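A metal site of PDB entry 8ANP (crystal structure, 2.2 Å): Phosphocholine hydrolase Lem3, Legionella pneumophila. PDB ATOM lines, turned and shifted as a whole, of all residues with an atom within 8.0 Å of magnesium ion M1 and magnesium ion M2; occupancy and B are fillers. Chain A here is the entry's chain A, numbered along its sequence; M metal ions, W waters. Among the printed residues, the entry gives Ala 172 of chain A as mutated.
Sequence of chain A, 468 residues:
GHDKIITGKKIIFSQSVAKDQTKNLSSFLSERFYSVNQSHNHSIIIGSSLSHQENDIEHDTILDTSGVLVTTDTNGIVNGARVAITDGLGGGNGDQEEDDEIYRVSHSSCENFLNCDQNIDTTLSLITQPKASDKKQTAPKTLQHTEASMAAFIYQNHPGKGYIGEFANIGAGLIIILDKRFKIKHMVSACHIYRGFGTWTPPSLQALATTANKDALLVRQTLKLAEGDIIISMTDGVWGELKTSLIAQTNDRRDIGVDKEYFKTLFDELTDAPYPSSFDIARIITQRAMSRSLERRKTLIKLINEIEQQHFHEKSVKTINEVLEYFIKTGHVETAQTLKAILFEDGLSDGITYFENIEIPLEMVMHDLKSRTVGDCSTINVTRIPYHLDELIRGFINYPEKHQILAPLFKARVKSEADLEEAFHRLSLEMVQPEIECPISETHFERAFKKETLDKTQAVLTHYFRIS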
ATOM      1  N   ILE A  62     -30.156  24.533  -2.774  1.00  0.00           N
ATOM      2  CA  ILE A  62     -28.705  24.511  -2.437  1.00  0.00           C
ATOM      3  C   ILE A  62     -27.936  24.960  -3.687  1.00  0.00           C
ATOM      4  O   ILE A  62     -28.071  24.307  -4.733  1.00  0.00           O
ATOM      5  CB  ILE A  62     -28.292  23.110  -1.929  1.00  0.00           C
ATOM      6  CG1 ILE A  62     -28.908  22.836  -0.558  1.00  0.00           C
ATOM      7  CG2 ILE A  62     -26.784  22.939  -1.915  1.00  0.00           C
ATOM      8  CD1 ILE A  62     -28.958  21.373  -0.172  1.00  0.00           C
ATOM      9  N   LEU A  63     -27.208  26.084  -3.576  1.00  0.00           N
ATOM     10  CA  LEU A  63     -26.517  26.744  -4.714  1.00  0.00           C
ATOM     11  C   LEU A  63     -25.022  26.399  -4.693  1.00  0.00           C
ATOM     12  O   LEU A  63     -24.291  26.915  -5.557  1.00  0.00           O
ATOM     13  CB  LEU A  63     -26.771  28.250  -4.634  1.00  0.00           C
ATOM     14  CG  LEU A  63     -28.232  28.678  -4.777  1.00  0.00           C
ATOM     15  CD1 LEU A  63     -28.372  30.193  -4.692  1.00  0.00           C
ATOM     16  CD2 LEU A  63     -28.832  28.164  -6.071  1.00  0.00           C
ATOM     17  N   ASP A  64     -24.609  25.534  -3.767  1.00  0.00           N
ATOM     18  CA  ASP A  64     -23.246  24.931  -3.717  1.00  0.00           C
ATOM     19  C   ASP A  64     -23.216  23.694  -4.621  1.00  0.00           C
ATOM     20  O   ASP A  64     -24.250  23.003  -4.717  1.00  0.00           O
ATOM     21  CB  ASP A  64     -22.848  24.504  -2.303  1.00  0.00           C
ATOM     22  CG  ASP A  64     -22.517  25.627  -1.336  1.00  0.00           C
ATOM     23  OD1 ASP A  64     -22.490  26.803  -1.757  1.00  0.00           O
ATOM     24  OD2 ASP A  64     -22.271  25.310  -0.167  1.00  0.00           O
ATOM     25  N   THR A  86     -17.910  24.687  -5.444  1.00  0.00           N
ATOM     26  CA  THR A  86     -18.395  25.999  -5.938  1.00  0.00           C
ATOM     27  C   THR A  86     -19.510  26.516  -5.029  1.00  0.00           C
ATOM     28  O   THR A  86     -20.229  25.682  -4.422  1.00  0.00           O
ATOM     29  CB  THR A  86     -18.822  25.899  -7.408  1.00  0.00           C
ATOM     30  OG1 THR A  86     -19.805  24.860  -7.528  1.00  0.00           O
ATOM     31  CG2 THR A  86     -17.671  25.588  -8.336  1.00  0.00           C
ATOM     32  N   ASP A  87     -19.604  27.832  -4.931  1.00  0.00           N
ATOM     33  CA  ASP A  87     -20.649  28.579  -4.174  1.00  0.00           C
ATOM     34  C   ASP A  87     -21.256  29.622  -5.131  1.00  0.00           C
ATOM     35  O   ASP A  87     -20.564  30.604  -5.429  1.00  0.00           O
ATOM     36  CB  ASP A  87     -20.050  29.193  -2.915  1.00  0.00           C
ATOM     37  CG  ASP A  87     -21.034  29.992  -2.068  1.00  0.00           C
ATOM     38  OD1 ASP A  87     -22.097  30.369  -2.590  1.00  0.00           O
ATOM     39  OD2 ASP A  87     -20.720  30.230  -0.879  1.00  0.00           O
ATOM     40  N   GLY A  88     -22.478  29.372  -5.607  1.00  0.00           N
ATOM     41  CA  GLY A  88     -23.248  30.333  -6.410  1.00  0.00           C
ATOM     42  C   GLY A  88     -23.534  31.591  -5.605  1.00  0.00           C
ATOM     43  O   GLY A  88     -24.032  31.460  -4.468  1.00  0.00           O
ATOM     44  N   LEU A  89     -23.210  32.759  -6.152  1.00  0.00           N
ATOM     45  CA  LEU A  89     -23.364  34.074  -5.477  1.00  0.00           C
ATOM     46  C   LEU A  89     -24.777  34.602  -5.735  1.00  0.00           C
ATOM     47  O   LEU A  89     -25.279  34.407  -6.858  1.00  0.00           O
ATOM     48  CB  LEU A  89     -22.277  35.037  -5.979  1.00  0.00           C
ATOM     49  CG  LEU A  89     -20.840  34.537  -5.863  1.00  0.00           C
ATOM     50  CD1 LEU A  89     -19.864  35.623  -6.264  1.00  0.00           C
ATOM     51  CD2 LEU A  89     -20.542  34.043  -4.455  1.00  0.00           C
ATOM     52  N   GLY A  90     -25.382  35.232  -4.719  1.00  0.00           N
ATOM     53  CA  GLY A  90     -26.779  35.731  -4.763  1.00  0.00           C
ATOM     54  C   GLY A  90     -27.771  34.604  -4.507  1.00  0.00           C
ATOM     55  O   GLY A  90     -27.327  33.508  -4.074  1.00  0.00           O
ATOM     56  N   GLY A  91     -29.049  34.848  -4.771  1.00  0.00           N
ATOM     57  CA  GLY A  91     -30.140  33.882  -4.572  1.00  0.00           C
ATOM     58  C   GLY A  91     -30.603  33.832  -3.125  1.00  0.00           C
ATOM     59  O   GLY A  91     -30.189  34.718  -2.346  1.00  0.00           O
ATOM     60  N   GLY A  92     -31.414  32.824  -2.784  1.00  0.00           N
ATOM     61  CA  GLY A  92     -32.031  32.651  -1.448  1.00  0.00           C
ATOM     62  C   GLY A  92     -33.040  33.755  -1.136  1.00  0.00           C
ATOM     63  O   GLY A  92     -33.182  34.089   0.056  1.00  0.00           O
ATOM     64  N   ILE A 102     -28.516  30.561 -11.194  1.00  0.00           N
ATOM     65  CA  ILE A 102     -27.297  30.586 -10.321  1.00  0.00           C
ATOM     66  C   ILE A 102     -26.774  29.150 -10.149  1.00  0.00           C
ATOM     67  O   ILE A 102     -25.538  28.972 -10.179  1.00  0.00           O
ATOM     68  CB  ILE A 102     -27.593  31.268  -8.966  1.00  0.00           C
ATOM     69  CG1 ILE A 102     -27.886  32.760  -9.147  1.00  0.00           C
ATOM     70  CG2 ILE A 102     -26.455  31.037  -7.982  1.00  0.00           C
ATOM     71  CD1 ILE A 102     -28.534  33.418  -7.954  1.00  0.00           C
ATOM     72  N   SER A 106     -23.001  27.493 -11.067  1.00  0.00           N
ATOM     73  CA  SER A 106     -22.336  26.777  -9.942  1.00  0.00           C
ATOM     74  C   SER A 106     -21.967  25.361 -10.375  1.00  0.00           C
ATOM     75  O   SER A 106     -20.807  24.960 -10.152  1.00  0.00           O
ATOM     76  CB  SER A 106     -23.212  26.756  -8.707  1.00  0.00           C
ATOM     77  OG  SER A 106     -22.607  25.957  -7.707  1.00  0.00           O
ATOM     78  N   GLU A 147     -22.870  34.341 -11.201  1.00  0.00           N
ATOM     79  CA  GLU A 147     -21.463  34.160 -10.739  1.00  0.00           C
ATOM     80  C   GLU A 147     -21.386  33.035  -9.703  1.00  0.00           C
ATOM     81  O   GLU A 147     -22.368  32.831  -8.962  1.00  0.00           O
ATOM     82  CB  GLU A 147     -20.937  35.463 -10.140  1.00  0.00           C
ATOM     83  CG  GLU A 147     -20.741  36.565 -11.166  1.00  0.00           C
ATOM     84  CD  GLU A 147     -19.927  37.747 -10.651  1.00  0.00           C
ATOM     85  OE1 GLU A 147     -18.913  38.077 -11.280  1.00  0.00           O
ATOM     86  OE2 GLU A 147     -20.313  38.330  -9.619  1.00  0.00           O
ATOM     87  N   ALA A 148     -20.237  32.350  -9.645  1.00  0.00           N
ATOM     88  CA  ALA A 148     -19.885  31.365  -8.599  1.00  0.00           C
ATOM     89  C   ALA A 148     -18.411  31.523  -8.204  1.00  0.00           C
ATOM     90  O   ALA A 148     -17.561  31.732  -9.092  1.00  0.00           O
ATOM     91  CB  ALA A 148     -20.172  29.974  -9.083  1.00  0.00           C
ATOM     92  N   SER A 149     -18.130  31.461  -6.893  1.00  0.00           N
ATOM     93  CA  SER A 149     -16.771  31.273  -6.333  1.00  0.00           C
ATOM     94  C   SER A 149     -16.372  29.808  -6.507  1.00  0.00           C
ATOM     95  O   SER A 149     -17.293  28.960  -6.589  1.00  0.00           O
ATOM     96  CB  SER A 149     -16.723  31.692  -4.886  1.00  0.00           C
ATOM     97  OG  SER A 149     -17.386  30.747  -4.069  1.00  0.00           O
ATOM     98  N   ALA A 172     -14.698  32.915  -1.278  1.00  0.00           N
ATOM     99  CA  ALA A 172     -14.752  32.705   0.187  1.00  0.00           C
ATOM    100  C   ALA A 172     -14.843  31.212   0.531  1.00  0.00           C
ATOM    101  O   ALA A 172     -15.201  30.901   1.670  1.00  0.00           O
ATOM    102  CB  ALA A 172     -15.895  33.484   0.792  1.00  0.00           C
ATOM    103  N   GLY A 173     -14.549  30.326  -0.429  1.00  0.00           N
ATOM    104  CA  GLY A 173     -14.219  28.917  -0.143  1.00  0.00           C
ATOM    105  C   GLY A 173     -12.895  28.824   0.587  1.00  0.00           C
ATOM    106  O   GLY A 173     -12.172  29.836   0.622  1.00  0.00           O
ATOM    107  N   PRO A 202     -16.992  38.025  -1.691  1.00  0.00           N
ATOM    108  CA  PRO A 202     -15.962  37.242  -2.374  1.00  0.00           C
ATOM    109  C   PRO A 202     -15.911  37.479  -3.882  1.00  0.00           C
ATOM    110  O   PRO A 202     -16.938  37.710  -4.520  1.00  0.00           O
ATOM    111  CB  PRO A 202     -16.373  35.790  -2.093  1.00  0.00           C
ATOM    112  CG  PRO A 202     -17.873  35.852  -1.881  1.00  0.00           C
ATOM    113  CD  PRO A 202     -18.117  37.203  -1.226  1.00  0.00           C
ATOM    114  N   MET A 234     -14.131  23.521   1.864  1.00  0.00           N
ATOM    115  CA  MET A 234     -15.383  23.974   2.522  1.00  0.00           C
ATOM    116  C   MET A 234     -15.860  25.278   1.873  1.00  0.00           C
ATOM    117  O   MET A 234     -15.005  26.149   1.613  1.00  0.00           O
ATOM    118  CB  MET A 234     -15.150  24.187   4.021  1.00  0.00           C
ATOM    119  CG  MET A 234     -14.915  22.908   4.810  1.00  0.00           C
ATOM    120  SD  MET A 234     -14.107  23.259   6.572  1.00  0.00           S
ATOM    121  CE  MET A 234     -12.347  24.102   6.394  1.00  0.00           C
ATOM    122  N   THR A 235     -17.162  25.401   1.627  1.00  0.00           N
ATOM    123  CA  THR A 235     -17.833  26.701   1.339  1.00  0.00           C
ATOM    124  C   THR A 235     -17.962  27.438   2.669  1.00  0.00           C
ATOM    125  O   THR A 235     -17.883  26.766   3.712  1.00  0.00           O
ATOM    126  CB  THR A 235     -19.157  26.521   0.587  1.00  0.00           C
ATOM    127  OG1 THR A 235     -20.090  25.787   1.383  1.00  0.00           O
ATOM    128  CG2 THR A 235     -18.962  25.813  -0.737  1.00  0.00           C
ATOM    129  N   ASP A 236     -18.123  28.759   2.646  1.00  0.00           N
ATOM    130  CA  ASP A 236     -18.181  29.611   3.863  1.00  0.00           C
ATOM    131  C   ASP A 236     -19.323  29.159   4.790  1.00  0.00           C
ATOM    132  O   ASP A 236     -19.252  29.473   5.988  1.00  0.00           O
ATOM    133  CB  ASP A 236     -18.294  31.097   3.524  1.00  0.00           C
ATOM    134  CG  ASP A 236     -19.353  31.440   2.491  1.00  0.00           C
ATOM    135  OD1 ASP A 236     -20.097  30.522   2.075  1.00  0.00           O
ATOM    136  OD2 ASP A 236     -19.432  32.623   2.104  1.00  0.00           O
ATOM    137  N   GLY A 237     -20.338  28.466   4.260  1.00  0.00           N
ATOM    138  CA  GLY A 237     -21.455  27.889   5.048  1.00  0.00           C
ATOM    139  C   GLY A 237     -20.974  26.967   6.150  1.00  0.00           C
ATOM    140  O   GLY A 237     -21.609  26.940   7.222  1.00  0.00           O
ATOM    141  N   VAL A 238     -19.899  26.205   5.904  1.00  0.00           N
ATOM    142  CA  VAL A 238     -19.279  25.283   6.908  1.00  0.00           C
ATOM    143  C   VAL A 238     -18.225  26.049   7.712  1.00  0.00           C
ATOM    144  O   VAL A 238     -18.447  26.215   8.930  1.00  0.00           O
ATOM    145  CB  VAL A 238     -18.700  24.017   6.235  1.00  0.00           C
ATOM    146  CG1 VAL A 238     -17.899  23.179   7.213  1.00  0.00           C
ATOM    147  CG2 VAL A 238     -19.790  23.185   5.592  1.00  0.00           C
ATOM    148  N   TRP A 239     -17.131  26.502   7.092  1.00  0.00           N
ATOM    149  CA  TRP A 239     -15.949  27.023   7.819  1.00  0.00           C
ATOM    150  C   TRP A 239     -16.262  28.370   8.490  1.00  0.00           C
ATOM    151  O   TRP A 239     -15.636  28.676   9.516  1.00  0.00           O
ATOM    152  CB  TRP A 239     -14.691  27.092   6.925  1.00  0.00           C
ATOM    153  CG  TRP A 239     -14.691  28.177   5.899  1.00  0.00           C
ATOM    154  CD1 TRP A 239     -15.027  28.056   4.585  1.00  0.00           C
ATOM    155  CD2 TRP A 239     -14.325  29.556   6.089  1.00  0.00           C
ATOM    156  NE1 TRP A 239     -14.895  29.264   3.941  1.00  0.00           N
ATOM    157  CE2 TRP A 239     -14.477  30.202   4.837  1.00  0.00           C
ATOM    158  CE3 TRP A 239     -13.892  30.319   7.184  1.00  0.00           C
ATOM    159  CZ2 TRP A 239     -14.216  31.566   4.664  1.00  0.00           C
ATOM    160  CZ3 TRP A 239     -13.624  31.659   7.012  1.00  0.00           C
ATOM    161  CH2 TRP A 239     -13.790  32.271   5.769  1.00  0.00           C
ATOM    162  N   GLY A 375     -27.644  31.274   8.540  1.00  0.00           N
ATOM    163  CA  GLY A 375     -27.085  30.091   7.859  1.00  0.00           C
ATOM    164  C   GLY A 375     -26.907  30.342   6.367  1.00  0.00           C
ATOM    165  O   GLY A 375     -26.920  31.511   5.957  1.00  0.00           O
ATOM    166  N   ASP A 376     -26.756  29.262   5.590  1.00  0.00           N
ATOM    167  CA  ASP A 376     -26.309  29.312   4.177  1.00  0.00           C
ATOM    168  C   ASP A 376     -26.244  27.876   3.634  1.00  0.00           C
ATOM    169  O   ASP A 376     -26.275  26.932   4.450  1.00  0.00           O
ATOM    170  CB  ASP A 376     -24.931  29.973   4.068  1.00  0.00           C
ATOM    171  CG  ASP A 376     -24.502  30.342   2.654  1.00  0.00           C
ATOM    172  OD1 ASP A 376     -25.366  30.383   1.776  1.00  0.00           O
ATOM    173  OD2 ASP A 376     -23.286  30.578   2.456  1.00  0.00           O
ATOM    174  N   CYS A 377     -26.167  27.735   2.308  1.00  0.00           N
ATOM    175  CA  CYS A 377     -25.665  26.509   1.626  1.00  0.00           C
ATOM    176  C   CYS A 377     -24.329  26.126   2.284  1.00  0.00           C
ATOM    177  O   CYS A 377     -23.460  27.003   2.403  1.00  0.00           O
ATOM    178  CB  CYS A 377     -25.469  26.748   0.127  1.00  0.00           C
ATOM    179  SG  CYS A 377     -26.889  27.554  -0.657  1.00  0.00           S
ATOM    180  N   SER A 378     -24.207  24.886   2.741  1.00  0.00           N
ATOM    181  CA  SER A 378     -23.068  24.385   3.553  1.00  0.00           C
ATOM    182  C   SER A 378     -22.546  23.086   2.937  1.00  0.00           C
ATOM    183  O   SER A 378     -23.303  22.090   2.933  1.00  0.00           O
ATOM    184  CB  SER A 378     -23.467  24.218   4.990  1.00  0.00           C
ATOM    185  OG  SER A 378     -23.926  25.443   5.539  1.00  0.00           O
ATOM    186  N   THR A 379     -21.325  23.114   2.397  1.00  0.00           N
ATOM    187  CA  THR A 379     -20.729  21.967   1.662  1.00  0.00           C
ATOM    188  C   THR A 379     -19.276  21.777   2.094  1.00  0.00           C
ATOM    189  O   THR A 379     -18.571  22.782   2.301  1.00  0.00           O
ATOM    190  CB  THR A 379     -20.859  22.156   0.140  1.00  0.00           C
ATOM    191  OG1 THR A 379     -22.215  22.514  -0.126  1.00  0.00           O
ATOM    192  CG2 THR A 379     -20.485  20.913  -0.634  1.00  0.00           C
HETATM  193 MG    MG M   1     -21.766  30.422   0.824  1.00  0.00          MG
HETATM  194 MG    MG M   2     -23.923  31.484  -2.298  1.00  0.00          MG
HETATM  195  O   HOH W   1     -25.770  32.252  -2.401  1.00  0.00           O
HETATM  196  O   HOH W   2     -21.829  32.415   0.929  1.00  0.00           O
HETATM  197  O   HOH W   3     -22.186  28.317   0.512  1.00  0.00           O
HETATM  198  O   HOH W   4     -23.028  33.805  -1.792  1.00  0.00           O
HETATM  199  O   HOH W   5     -23.610  30.826  -0.266  1.00  0.00           O
HETATM  200  O   HOH W   6     -24.286  28.989  -2.414  1.00  0.00           O
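Water W3 lies within hydrogen-bond range of the backbone carbonyl oxygen (O) of Cys 377 (2.6 Å), the side-chain carboxylate (OD1) of Asp 64 (2.7 Å) and the side-chain hydroxyl (OG1) of Thr 235 (3.4 Å). Water W6 lies within hydrogen-bond range of OD1 of Asp 64 (2.9 Å) and SG of Cys 377 (3.5 Å).
Magnesium ion M1 is bound by water W2 (2.0 Å), the side-chain carboxylate of Asp 87 (2.0 Å), the side-chain carboxylate of Asp 236 (2.1 Å), water W3 (2.2 Å), water W5 (2.2 Å) and the side-chain carboxylate of Asp 376 (2.2 Å). Magnesium ion M1 has six donor atoms within binding distance.
Magnesium ion M2 is bound by water W1 (2.0 Å), water W5 (2.2 Å), the side-chain carboxylate (OD1) of Asp 87 (2.2 Å), the backbone carbonyl oxygen (O) of Gly 88 (2.2 Å), water W6 (2.5 Å) and water W4 (2.5 Å). Magnesium ion M2 has six donor atoms within binding distance.
The nearest printed residue that does not touch magnesium ion M1 is Cys 377 (4.1 Å).
N of Gly 88 sits at hydrogen-bond distance from O of Leu 63, at 3.1 Å. OG of Ser 378 is in hydrogen-bond range of O of Asp 376 (3.0 Å). The backbone carbonyl oxygen (O) of Asp 87 sits at hydrogen-bond distance from the backbone NH (N) of Ser 149.
Within 4 Å of magnesium ion M2: Asp 87 and Gly 88. The nearest printed residue that does not touch magnesium ion M2 is Leu 89 (4.1 Å).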
